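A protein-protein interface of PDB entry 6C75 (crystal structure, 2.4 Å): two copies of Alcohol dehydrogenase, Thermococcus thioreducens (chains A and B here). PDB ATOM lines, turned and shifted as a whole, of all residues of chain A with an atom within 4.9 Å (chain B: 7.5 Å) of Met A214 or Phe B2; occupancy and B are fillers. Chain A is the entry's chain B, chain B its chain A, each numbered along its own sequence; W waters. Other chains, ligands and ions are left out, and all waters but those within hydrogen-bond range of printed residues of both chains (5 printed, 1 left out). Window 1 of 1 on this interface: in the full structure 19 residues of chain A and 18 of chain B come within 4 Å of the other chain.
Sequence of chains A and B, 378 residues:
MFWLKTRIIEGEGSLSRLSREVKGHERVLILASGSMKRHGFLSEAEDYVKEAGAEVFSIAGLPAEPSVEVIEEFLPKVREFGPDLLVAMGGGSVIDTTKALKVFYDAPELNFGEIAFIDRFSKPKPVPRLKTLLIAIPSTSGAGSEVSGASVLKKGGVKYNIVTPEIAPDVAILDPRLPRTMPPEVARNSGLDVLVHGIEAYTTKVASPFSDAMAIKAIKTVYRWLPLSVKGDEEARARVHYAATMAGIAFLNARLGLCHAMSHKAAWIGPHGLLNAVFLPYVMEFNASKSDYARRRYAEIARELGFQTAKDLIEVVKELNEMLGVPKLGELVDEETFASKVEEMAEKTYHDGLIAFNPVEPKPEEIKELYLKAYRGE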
ATOM      1  N   LEU A   4      11.029  30.077  24.220  1.00  0.00           N
ATOM      2  CA  LEU A   4      12.127  30.053  23.270  1.00  0.00           C
ATOM      3  C   LEU A   4      12.060  31.341  22.479  1.00  0.00           C
ATOM      4  O   LEU A   4      11.089  31.576  21.765  1.00  0.00           O
ATOM      5  CB  LEU A   4      11.984  28.849  22.331  1.00  0.00           C
ATOM      6  CG  LEU A   4      13.109  28.587  21.325  1.00  0.00           C
ATOM      7  CD1 LEU A   4      14.434  28.324  22.027  1.00  0.00           C
ATOM      8  CD2 LEU A   4      12.743  27.416  20.424  1.00  0.00           C
ATOM      9  N   THR A   6      14.519  32.378  20.502  1.00  0.00           N
ATOM     10  CA  THR A   6      15.269  32.197  19.260  1.00  0.00           C
ATOM     11  C   THR A   6      14.407  31.499  18.226  1.00  0.00           C
ATOM     12  O   THR A   6      13.734  30.519  18.539  1.00  0.00           O
ATOM     13  CB  THR A   6      16.513  31.325  19.495  1.00  0.00           C
ATOM     14  OG1 THR A   6      17.296  31.896  20.540  1.00  0.00           O
ATOM     15  CG2 THR A   6      17.346  31.223  18.240  1.00  0.00           C
ATOM     16  N   ARG A   7      14.540  31.919  16.975  1.00  0.00           N
ATOM     17  CA  ARG A   7      13.886  31.237  15.866  1.00  0.00           C
ATOM     18  C   ARG A   7      14.905  30.422  15.080  1.00  0.00           C
ATOM     19  O   ARG A   7      15.942  30.938  14.668  1.00  0.00           O
ATOM     20  CB  ARG A   7      13.200  32.245  14.944  1.00  0.00           C
ATOM     21  CG  ARG A   7      12.617  31.627  13.687  1.00  0.00           C
ATOM     22  CD  ARG A   7      11.735  32.619  12.941  1.00  0.00           C
ATOM     23  NE  ARG A   7      12.316  33.962  12.897  1.00  0.00           N
ATOM     24  CZ  ARG A   7      13.009  34.450  11.871  1.00  0.00           C
ATOM     25  NH1 ARG A   7      13.242  33.695  10.802  1.00  0.00           N
ATOM     26  NH2 ARG A   7      13.486  35.686  11.924  1.00  0.00           N
ATOM     27  N   ILE A   8      14.572  29.162  14.823  1.00  0.00           N
ATOM     28  CA  ILE A   8      15.556  28.194  14.381  1.00  0.00           C
ATOM     29  C   ILE A   8      15.340  27.833  12.911  1.00  0.00           C
ATOM     30  O   ILE A   8      14.264  27.372  12.521  1.00  0.00           O
ATOM     31  CB  ILE A   8      15.510  26.934  15.259  1.00  0.00           C
ATOM     32  CG1 ILE A   8      16.062  27.252  16.650  1.00  0.00           C
ATOM     33  CG2 ILE A   8      16.312  25.807  14.627  1.00  0.00           C
ATOM     34  CD1 ILE A   8      15.569  26.314  17.726  1.00  0.00           C
ATOM     35  N   GLU A  10      16.784  25.324  10.269  1.00  0.00           N
ATOM     36  CA  GLU A  10      17.622  24.158  10.046  1.00  0.00           C
ATOM     37  C   GLU A  10      17.547  23.736   8.584  1.00  0.00           C
ATOM     38  O   GLU A  10      16.740  24.271   7.825  1.00  0.00           O
ATOM     39  CB  GLU A  10      17.201  23.014  10.977  1.00  0.00           C
ATOM     40  CG  GLU A  10      16.247  21.999  10.367  1.00  0.00           C
ATOM     41  CD  GLU A  10      14.798  22.415  10.491  1.00  0.00           C
ATOM     42  OE1 GLU A  10      14.534  23.480  11.083  1.00  0.00           O
ATOM     43  OE2 GLU A  10      13.927  21.695   9.966  1.00  0.00           O
ATOM     44  N   PHE A 210       7.954  19.898  28.871  1.00  0.00           N
ATOM     45  CA  PHE A 210       8.337  20.536  27.612  1.00  0.00           C
ATOM     46  C   PHE A 210       9.842  20.462  27.390  1.00  0.00           C
ATOM     47  O   PHE A 210      10.288  19.987  26.351  1.00  0.00           O
ATOM     48  CB  PHE A 210       7.867  21.993  27.585  1.00  0.00           C
ATOM     49  CG  PHE A 210       6.385  22.150  27.785  1.00  0.00           C
ATOM     50  CD1 PHE A 210       5.507  21.924  26.738  1.00  0.00           C
ATOM     51  CD2 PHE A 210       5.863  22.348  29.055  1.00  0.00           C
ATOM     52  CE1 PHE A 210       4.140  21.944  26.942  1.00  0.00           C
ATOM     53  CE2 PHE A 210       4.497  22.352  29.270  1.00  0.00           C
ATOM     54  CZ  PHE A 210       3.635  22.135  28.215  1.00  0.00           C
ATOM     55  N   SER A 211      10.614  20.760  28.429  1.00  0.00           N
ATOM     56  CA  SER A 211      12.068  20.646  28.346  1.00  0.00           C
ATOM     57  C   SER A 211      12.515  19.183  28.314  1.00  0.00           C
ATOM     58  O   SER A 211      13.426  18.829  27.563  1.00  0.00           O
ATOM     59  CB  SER A 211      12.739  21.397  29.503  1.00  0.00           C
ATOM     60  OG  SER A 211      12.778  20.611  30.679  1.00  0.00           O
ATOM     61  N   ASP A 212      11.787  18.325  29.027  1.00  0.00           N
ATOM     62  CA  ASP A 212      12.001  16.876  28.966  1.00  0.00           C
ATOM     63  C   ASP A 212      11.917  16.329  27.536  1.00  0.00           C
ATOM     64  O   ASP A 212      12.696  15.450  27.155  1.00  0.00           O
ATOM     65  CB  ASP A 212      10.986  16.144  29.852  1.00  0.00           C
ATOM     66  CG  ASP A 212      11.331  16.226  31.333  1.00  0.00           C
ATOM     67  OD1 ASP A 212      12.463  16.638  31.657  1.00  0.00           O
ATOM     68  OD2 ASP A 212      10.469  15.883  32.172  1.00  0.00           O
ATOM     69  N   ALA A 213      10.940  16.802  26.767  1.00  0.00           N
ATOM     70  CA  ALA A 213      10.756  16.331  25.396  1.00  0.00           C
ATOM     71  C   ALA A 213      11.998  16.576  24.533  1.00  0.00           C
ATOM     72  O   ALA A 213      12.344  15.743  23.699  1.00  0.00           O
ATOM     73  CB  ALA A 213       9.545  17.001  24.770  1.00  0.00           C
ATOM     74  N   MET A 214      12.677  17.704  24.752  1.00  0.00           N
ATOM     75  CA  MET A 214      13.873  18.046  23.982  1.00  0.00           C
ATOM     76  C   MET A 214      15.111  17.311  24.504  1.00  0.00           C
ATOM     77  O   MET A 214      15.934  16.833  23.724  1.00  0.00           O
ATOM     78  CB  MET A 214      14.119  19.555  24.018  1.00  0.00           C
ATOM     79  CG  MET A 214      13.062  20.383  23.300  1.00  0.00           C
ATOM     80  SD  MET A 214      13.022  20.068  21.524  1.00  0.00           S
ATOM     81  CE  MET A 214      12.146  21.513  20.938  1.00  0.00           C
ATOM     82  N   ALA A 215      15.221  17.187  25.821  1.00  0.00           N
ATOM     83  CA  ALA A 215      16.340  16.462  26.423  1.00  0.00           C
ATOM     84  C   ALA A 215      16.383  15.000  25.972  1.00  0.00           C
ATOM     85  O   ALA A 215      17.438  14.491  25.584  1.00  0.00           O
ATOM     86  CB  ALA A 215      16.268  16.545  27.945  1.00  0.00           C
ATOM     87  N   ILE A 216      15.257  14.307  26.118  1.00  0.00           N
ATOM     88  CA  ILE A 216      15.186  12.880  25.823  1.00  0.00           C
ATOM     89  C   ILE A 216      15.610  12.602  24.384  1.00  0.00           C
ATOM     90  O   ILE A 216      16.402  11.701  24.114  1.00  0.00           O
ATOM     91  CB  ILE A 216      13.758  12.352  26.033  1.00  0.00           C
ATOM     92  CG1 ILE A 216      13.496  12.128  27.519  1.00  0.00           C
ATOM     93  CG2 ILE A 216      13.546  11.059  25.263  1.00  0.00           C
ATOM     94  CD1 ILE A 216      14.433  11.121  28.151  1.00  0.00           C
ATOM     95  N   LYS A 217      15.056  13.368  23.459  1.00  0.00           N
ATOM     96  CA  LYS A 217      15.328  13.164  22.047  1.00  0.00           C
ATOM     97  C   LYS A 217      16.801  13.444  21.722  1.00  0.00           C
ATOM     98  O   LYS A 217      17.438  12.687  20.981  1.00  0.00           O
ATOM     99  CB  LYS A 217      14.413  14.063  21.220  1.00  0.00           C
ATOM    100  CG  LYS A 217      14.730  14.095  19.738  1.00  0.00           C
ATOM    101  CD  LYS A 217      13.955  13.038  18.975  1.00  0.00           C
ATOM    102  CE  LYS A 217      13.682  13.496  17.554  1.00  0.00           C
ATOM    103  NZ  LYS A 217      13.625  12.335  16.628  1.00  0.00           N
ATOM    104  N   ALA A 218      17.352  14.511  22.302  1.00  0.00           N
ATOM    105  CA  ALA A 218      18.777  14.803  22.153  1.00  0.00           C
ATOM    106  C   ALA A 218      19.635  13.630  22.641  1.00  0.00           C
ATOM    107  O   ALA A 218      20.561  13.208  21.950  1.00  0.00           O
ATOM    108  CB  ALA A 218      19.144  16.079  22.897  1.00  0.00           C
ATOM    109  N   MET A 246      18.626  20.989  20.353  1.00  0.00           N
ATOM    110  CA  MET A 246      17.587  20.421  21.206  1.00  0.00           C
ATOM    111  C   MET A 246      17.995  20.471  22.679  1.00  0.00           C
ATOM    112  O   MET A 246      17.224  20.907  23.531  1.00  0.00           O
ATOM    113  CB  MET A 246      17.297  18.978  20.802  1.00  0.00           C
ATOM    114  CG  MET A 246      16.288  18.840  19.677  1.00  0.00           C
ATOM    115  SD  MET A 246      16.113  17.125  19.143  1.00  0.00           S
ATOM    116  CE  MET A 246      16.329  17.308  17.379  1.00  0.00           C
ATOM    117  N   ALA A 247      19.196  19.992  22.986  1.00  0.00           N
ATOM    118  CA  ALA A 247      19.689  20.019  24.359  1.00  0.00           C
ATOM    119  C   ALA A 247      19.864  21.457  24.851  1.00  0.00           C
ATOM    120  O   ALA A 247      19.644  21.755  26.025  1.00  0.00           O
ATOM    121  CB  ALA A 247      21.002  19.265  24.453  1.00  0.00           C
ATOM    122  N   ILE A 249      17.928  23.984  23.868  1.00  0.00           N
ATOM    123  CA  ILE A 249      16.575  24.401  24.215  1.00  0.00           C
ATOM    124  C   ILE A 249      16.174  23.868  25.591  1.00  0.00           C
ATOM    125  O   ILE A 249      15.586  24.593  26.400  1.00  0.00           O
ATOM    126  CB  ILE A 249      15.550  23.927  23.174  1.00  0.00           C
ATOM    127  CG1 ILE A 249      15.776  24.639  21.844  1.00  0.00           C
ATOM    128  CG2 ILE A 249      14.141  24.213  23.659  1.00  0.00           C
ATOM    129  CD1 ILE A 249      15.109  23.954  20.673  1.00  0.00           C
ATOM    130  N   ALA A 250      16.609  22.651  25.900  1.00  0.00           N
ATOM    131  CA  ALA A 250      16.267  22.013  27.165  1.00  0.00           C
ATOM    132  C   ALA A 250      16.891  22.703  28.383  1.00  0.00           C
ATOM    133  O   ALA A 250      16.215  22.891  29.399  1.00  0.00           O
ATOM    134  CB  ALA A 250      16.652  20.544  27.136  1.00  0.00           C
ATOM    135  N   MET B   1      12.145  24.832   9.731  1.00  0.00           N
ATOM    136  CA  MET B   1      12.080  25.987  10.675  1.00  0.00           C
ATOM    137  C   MET B   1      11.298  25.620  11.932  1.00  0.00           C
ATOM    138  O   MET B   1      10.288  24.926  11.856  1.00  0.00           O
ATOM    139  CB  MET B   1      11.432  27.191   9.994  1.00  0.00           C
ATOM    140  CG  MET B   1      11.416  28.438  10.859  1.00  0.00           C
ATOM    141  SD  MET B   1      10.705  29.862  10.015  1.00  0.00           S
ATOM    142  CE  MET B   1      12.162  30.539   9.212  1.00  0.00           C
ATOM    143  N   PHE B   2      11.763  26.094  13.085  1.00  0.00           N
ATOM    144  CA  PHE B   2      11.044  25.900  14.344  1.00  0.00           C
ATOM    145  C   PHE B   2      11.003  27.194  15.133  1.00  0.00           C
ATOM    146  O   PHE B   2      11.988  27.913  15.204  1.00  0.00           O
ATOM    147  CB  PHE B   2      11.720  24.816  15.183  1.00  0.00           C
ATOM    148  CG  PHE B   2      10.993  24.492  16.456  1.00  0.00           C
ATOM    149  CD1 PHE B   2       9.915  23.621  16.450  1.00  0.00           C
ATOM    150  CD2 PHE B   2      11.438  24.988  17.669  1.00  0.00           C
ATOM    151  CE1 PHE B   2       9.250  23.309  17.622  1.00  0.00           C
ATOM    152  CE2 PHE B   2      10.792  24.662  18.848  1.00  0.00           C
ATOM    153  CZ  PHE B   2       9.699  23.817  18.825  1.00  0.00           C
ATOM    154  N   TRP B   3       9.838  27.520  15.676  1.00  0.00           N
ATOM    155  CA  TRP B   3       9.694  28.709  16.505  1.00  0.00           C
ATOM    156  C   TRP B   3       8.499  28.565  17.438  1.00  0.00           C
ATOM    157  O   TRP B   3       7.634  27.714  17.239  1.00  0.00           O
ATOM    158  CB  TRP B   3       9.541  29.961  15.630  1.00  0.00           C
ATOM    159  CG  TRP B   3       8.291  29.962  14.821  1.00  0.00           C
ATOM    160  CD1 TRP B   3       8.047  29.228  13.697  1.00  0.00           C
ATOM    161  CD2 TRP B   3       7.059  30.610  15.152  1.00  0.00           C
ATOM    162  NE1 TRP B   3       6.744  29.393  13.297  1.00  0.00           N
ATOM    163  CE2 TRP B   3       6.111  30.228  14.180  1.00  0.00           C
ATOM    164  CE3 TRP B   3       6.665  31.485  16.168  1.00  0.00           C
ATOM    165  CZ2 TRP B   3       4.788  30.675  14.207  1.00  0.00           C
ATOM    166  CZ3 TRP B   3       5.345  31.922  16.197  1.00  0.00           C
ATOM    167  CH2 TRP B   3       4.423  31.509  15.231  1.00  0.00           C
ATOM    168  N   LEU B   4       8.511  29.335  18.514  1.00  0.00           N
ATOM    169  CA  LEU B   4       7.421  29.331  19.479  1.00  0.00           C
ATOM    170  C   LEU B   4       7.293  30.722  20.093  1.00  0.00           C
ATOM    171  O   LEU B   4       8.191  31.178  20.803  1.00  0.00           O
ATOM    172  CB  LEU B   4       7.685  28.291  20.574  1.00  0.00           C
ATOM    173  CG  LEU B   4       6.614  28.204  21.660  1.00  0.00           C
ATOM    174  CD1 LEU B   4       5.433  27.379  21.183  1.00  0.00           C
ATOM    175  CD2 LEU B   4       7.182  27.632  22.947  1.00  0.00           C
ATOM    176  N   SER B 208      10.083  18.670  11.203  1.00  0.00           N
ATOM    177  CA  SER B 208      11.482  18.720  11.610  1.00  0.00           C
ATOM    178  C   SER B 208      11.708  17.833  12.830  1.00  0.00           C
ATOM    179  O   SER B 208      10.755  17.414  13.476  1.00  0.00           O
ATOM    180  CB  SER B 208      11.889  20.157  11.927  1.00  0.00           C
ATOM    181  OG  SER B 208      11.461  20.523  13.223  1.00  0.00           O
ATOM    182  N   PRO B 209      12.977  17.538  13.138  1.00  0.00           N
ATOM    183  CA  PRO B 209      13.371  16.896  14.389  1.00  0.00           C
ATOM    184  C   PRO B 209      12.777  17.586  15.602  1.00  0.00           C
ATOM    185  O   PRO B 209      12.605  16.964  16.652  1.00  0.00           O
ATOM    186  CB  PRO B 209      14.892  17.058  14.399  1.00  0.00           C
ATOM    187  CG  PRO B 209      15.266  17.167  12.965  1.00  0.00           C
ATOM    188  CD  PRO B 209      14.140  17.918  12.324  1.00  0.00           C
ATOM    189  N   PHE B 210      12.628  18.900  15.501  1.00  0.00           N
ATOM    190  CA  PHE B 210      12.299  19.716  16.650  1.00  0.00           C
ATOM    191  C   PHE B 210      10.832  19.556  16.996  1.00  0.00           C
ATOM    192  O   PHE B 210      10.486  19.272  18.141  1.00  0.00           O
ATOM    193  CB  PHE B 210      12.625  21.177  16.362  1.00  0.00           C
ATOM    194  CG  PHE B 210      14.093  21.450  16.250  1.00  0.00           C
ATOM    195  CD1 PHE B 210      14.863  21.625  17.385  1.00  0.00           C
ATOM    196  CD2 PHE B 210      14.714  21.478  15.019  1.00  0.00           C
ATOM    197  CE1 PHE B 210      16.223  21.846  17.293  1.00  0.00           C
ATOM    198  CE2 PHE B 210      16.066  21.742  14.915  1.00  0.00           C
ATOM    199  CZ  PHE B 210      16.828  21.896  16.057  1.00  0.00           C
ATOM    200  N   SER B 211       9.989  19.573  15.973  1.00  0.00           N
ATOM    201  CA  SER B 211       8.566  19.308  16.163  1.00  0.00           C
ATOM    202  C   SER B 211       8.317  17.845  16.507  1.00  0.00           C
ATOM    203  O   SER B 211       7.456  17.544  17.327  1.00  0.00           O
ATOM    204  CB  SER B 211       7.773  19.694  14.916  1.00  0.00           C
ATOM    205  OG  SER B 211       8.236  18.986  13.777  1.00  0.00           O
ATOM    206  N   ASP B 212       9.080  16.946  15.891  1.00  0.00           N
ATOM    207  CA  ASP B 212       8.997  15.516  16.194  1.00  0.00           C
ATOM    208  C   ASP B 212       9.136  15.229  17.686  1.00  0.00           C
ATOM    209  O   ASP B 212       8.558  14.269  18.189  1.00  0.00           O
ATOM    210  CB  ASP B 212      10.094  14.741  15.463  1.00  0.00           C
ATOM    211  CG  ASP B 212       9.908  14.725  13.964  1.00  0.00           C
ATOM    212  OD1 ASP B 212       8.854  15.190  13.464  1.00  0.00           O
ATOM    213  OD2 ASP B 212      10.849  14.276  13.282  1.00  0.00           O
ATOM    214  N   ALA B 213      10.050  15.936  18.340  1.00  0.00           N
ATOM    215  CA  ALA B 213      10.304  15.726  19.760  1.00  0.00           C
ATOM    216  C   ALA B 213       9.048  15.974  20.586  1.00  0.00           C
ATOM    217  O   ALA B 213       8.846  15.339  21.621  1.00  0.00           O
ATOM    218  CB  ALA B 213      11.425  16.639  20.231  1.00  0.00           C
ATOM    219  N   MET B 214       8.342  17.047  20.246  1.00  0.00           N
ATOM    220  CA  MET B 214       7.114  17.418  20.940  1.00  0.00           C
ATOM    221  C   MET B 214       6.009  16.443  20.573  1.00  0.00           C
ATOM    222  O   MET B 214       5.256  15.998  21.436  1.00  0.00           O
ATOM    223  CB  MET B 214       6.694  18.842  20.557  1.00  0.00           C
ATOM    224  CG  MET B 214       7.583  19.937  21.137  1.00  0.00           C
ATOM    225  SD  MET B 214       7.490  20.027  22.935  1.00  0.00           S
ATOM    226  CE  MET B 214       8.955  20.982  23.314  1.00  0.00           C
ATOM    227  N   LYS B 217       6.521  12.752  22.229  1.00  0.00           N
ATOM    228  CA  LYS B 217       6.214  12.797  23.654  1.00  0.00           C
ATOM    229  C   LYS B 217       4.708  12.935  23.875  1.00  0.00           C
ATOM    230  O   LYS B 217       4.144  12.302  24.761  1.00  0.00           O
ATOM    231  CB  LYS B 217       6.957  13.953  24.323  1.00  0.00           C
ATOM    232  CG  LYS B 217       6.749  14.040  25.827  1.00  0.00           C
ATOM    233  CD  LYS B 217       7.480  12.930  26.563  1.00  0.00           C
ATOM    234  CE  LYS B 217       8.349  13.473  27.691  1.00  0.00           C
ATOM    235  NZ  LYS B 217       7.537  14.114  28.756  1.00  0.00           N
ATOM    236  N   ILE B 249       2.427  22.695  19.922  1.00  0.00           N
ATOM    237  CA  ILE B 249       3.726  23.222  19.509  1.00  0.00           C
ATOM    238  C   ILE B 249       4.208  22.509  18.247  1.00  0.00           C
ATOM    239  O   ILE B 249       4.799  23.122  17.357  1.00  0.00           O
ATOM    240  CB  ILE B 249       4.775  23.032  20.622  1.00  0.00           C
ATOM    241  CG1 ILE B 249       4.451  23.947  21.806  1.00  0.00           C
ATOM    242  CG2 ILE B 249       6.181  23.288  20.093  1.00  0.00           C
ATOM    243  CD1 ILE B 249       5.292  23.681  23.035  1.00  0.00           C
ATOM    244  N   ALA B 250       3.979  21.202  18.197  1.00  0.00           N
ATOM    245  CA  ALA B 250       4.397  20.399  17.056  1.00  0.00           C
ATOM    246  C   ALA B 250       3.695  20.836  15.762  1.00  0.00           C
ATOM    247  O   ALA B 250       4.345  21.008  14.736  1.00  0.00           O
ATOM    248  CB  ALA B 250       4.153  18.922  17.332  1.00  0.00           C
ATOM    249  N   PHE B 251       2.381  21.036  15.808  1.00  0.00           N
ATOM    250  CA  PHE B 251       1.634  21.314  14.585  1.00  0.00           C
ATOM    251  C   PHE B 251       1.567  22.809  14.258  1.00  0.00           C
ATOM    252  O   PHE B 251       1.476  23.180  13.095  1.00  0.00           O
ATOM    253  CB  PHE B 251       0.240  20.647  14.603  1.00  0.00           C
ATOM    254  CG  PHE B 251      -0.838  21.461  15.270  1.00  0.00           C
ATOM    255  CD1 PHE B 251      -1.305  22.630  14.687  1.00  0.00           C
ATOM    256  CD2 PHE B 251      -1.569  20.921  16.318  1.00  0.00           C
ATOM    257  CE1 PHE B 251      -2.290  23.382  15.308  1.00  0.00           C
ATOM    258  CE2 PHE B 251      -2.579  21.649  16.930  1.00  0.00           C
ATOM    259  CZ  PHE B 251      -2.935  22.884  16.429  1.00  0.00           C
ATOM    260  N   LEU B 252       1.871  23.651  15.237  1.00  0.00           N
ATOM    261  CA  LEU B 252       2.243  25.027  14.945  1.00  0.00           C
ATOM    262  C   LEU B 252       3.324  25.050  13.873  1.00  0.00           C
ATOM    263  O   LEU B 252       3.221  25.785  12.895  1.00  0.00           O
ATOM    264  CB  LEU B 252       2.744  25.726  16.205  1.00  0.00           C
ATOM    265  CG  LEU B 252       3.423  27.081  16.001  1.00  0.00           C
ATOM    266  CD1 LEU B 252       2.459  28.085  15.384  1.00  0.00           C
ATOM    267  CD2 LEU B 252       3.973  27.612  17.319  1.00  0.00           C
ATOM    268  N   ASN B 253       4.294  24.153  14.002  1.00  0.00           N
ATOM    269  CA  ASN B 253       5.499  24.188  13.176  1.00  0.00           C
ATOM    270  C   ASN B 253       5.434  23.208  11.995  1.00  0.00           C
ATOM    271  O   ASN B 253       5.838  23.542  10.879  1.00  0.00           O
ATOM    272  CB  ASN B 253       6.736  23.891  14.033  1.00  0.00           C
ATOM    273  CG  ASN B 253       7.106  25.045  14.948  1.00  0.00           C
ATOM    274  OD1 ASN B 253       7.789  25.975  14.533  1.00  0.00           O
ATOM    275  ND2 ASN B 253       6.762  24.928  16.229  1.00  0.00           N
ATOM    276  N   ALA B 254       4.919  22.008  12.242  1.00  0.00           N
ATOM    277  CA  ALA B 254       4.902  20.950  11.232  1.00  0.00           C
ATOM    278  C   ALA B 254       3.598  20.948  10.424  1.00  0.00           C
ATOM    279  O   ALA B 254       3.525  20.349   9.351  1.00  0.00           O
ATOM    280  CB  ALA B 254       5.117  19.594  11.892  1.00  0.00           C
HETATM  281  O   HOH W   1      14.219  25.800   8.022  1.00  0.00           O
HETATM  282  O   HOH W   2      10.767  13.756  22.746  1.00  0.00           O
HETATM  283  O   HOH W   3       9.210  13.660  31.303  1.00  0.00           O
HETATM  284  O   HOH W   4       8.503  30.923  23.571  1.00  0.00           O
HETATM  285  O   HOH W   5      11.084  30.467  19.186  1.00  0.00           O
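The backbone carbonyl oxygen (O) of Leu A4 sits close to the backbone carbonyl oxygen (O) of Leu B4 (3.1 Å).
OE1 of Glu A10 is in hydrogen-bond range of N of Met B1 (3.1 Å).
The backbone NH (N) of Phe B2 is in hydrogen-bond range of the backbone carbonyl oxygen (O) of Ile A8 (2.9 Å).
The side-chain hydroxyl (OG) of Ser B208 lies close to the backbone NH (N) of Phe B210 (3.0 Å).
The backbone carbonyl oxygen of Ser B208 sits at hydrogen-bond distance from the side-chain hydroxyl of Ser B211 (3.0 Å).
Among the printed residues, merely in contact across the chains: Ile A8 with Met B1 (3.2 Å), Glu A10 with Ser B208 (3.2 Å), Met A246 with Pro B209 (3.3 Å), Phe A210 with Met B214 (3.5 Å), Ala A213 with Ala B213 (3.6 Å), Arg A7 with Met B1 (3.7 Å), Leu A4 with Phe B2 (3.7 Å), Lys A217 with Pro B209 (3.7 Å), Met A246 with Phe B210 (3.8 Å), Arg A7 with Phe B2 (3.8 Å), Met A214 with Phe B210 (3.9 Å), Met A214 with Phe B2 (3.97 Å) and Met A214 with Ala B213 (3.998 Å).
Of the printed residues of chain B, Met A214 touches Phe B2 (3.97 Å), Phe B210 (3.9 Å) and Ala B213 (3.998 Å).
Phe B2 touches four residues of chain A.
Of the printed residues of chain A, Ala B213 touches Ala A213 and Met A214.
Printed residues of chain A within 4 Å of Met B214: Phe A210.
Printed residues of chain B within 4 Å of Phe A210: Met B214 (3.5 Å).
Printed residues of chain B within 4 Å of Arg A7: Met B1 (3.7 Å) and Phe B2 (3.8 Å).
Of the printed residues of chain A, Pro B209 touches Lys A217 (3.7 Å) and Met A246 (3.3 Å).
The nearest printed residue of chain B that does not touch Met A214 is Met B214 (4.01 Å).
Of the 18 printed residues of chain B, 8 touch a printed residue of chain A.
Of the 18 printed residues of chain A, 9 touch a printed residue of chain B.
Along chain A the printed residues that touch a printed residue of chain B span positions 4 to 246.
Among the printed residues, no Asp or Glu carboxylate lies within 4 Å of a Lys or Arg side-chain nitrogen of the other chain.
Leu A4 touches its own counterpart, Leu B4.
Phe A210 touches Met B214, and with the chains exchanged Met A214 touches Phe B210.
Ala A213 touches its own counterpart, Ala B213.
Met A214 touches Ala B213, but with the chains exchanged Ala A213 does not touch Met B214 (4.1 Å).
Positions printed for both chains: 4, 210, 211, 212, 213, 214, 217, 249 and 250.
Water W3 lies within hydrogen-bond range of OD2 of Asp A212 (2.7 Å) and NZ of Lys B217 (3.1 Å).
Water W2 lies within hydrogen-bond range of the backbone carbonyl oxygen of Ala A213 (2.7 Å) and the backbone carbonyl oxygen of Ala B213 (2.7 Å).
Water W5 lies within hydrogen-bond range of the backbone carbonyl oxygen of Thr A6 (2.7 Å), the backbone carbonyl oxygen of Leu A4 (2.8 Å) and the backbone NH of Leu B4 (2.9 Å).
Water W4 lies within hydrogen-bond range of the backbone NH (N) of Leu A4 (2.7 Å) and the backbone carbonyl oxygen (O) of Leu B4 (2.8 Å).
Water W1 lies within hydrogen-bond range of N of Met B1 (2.9 Å) and O of Glu A10 (3.0 Å).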
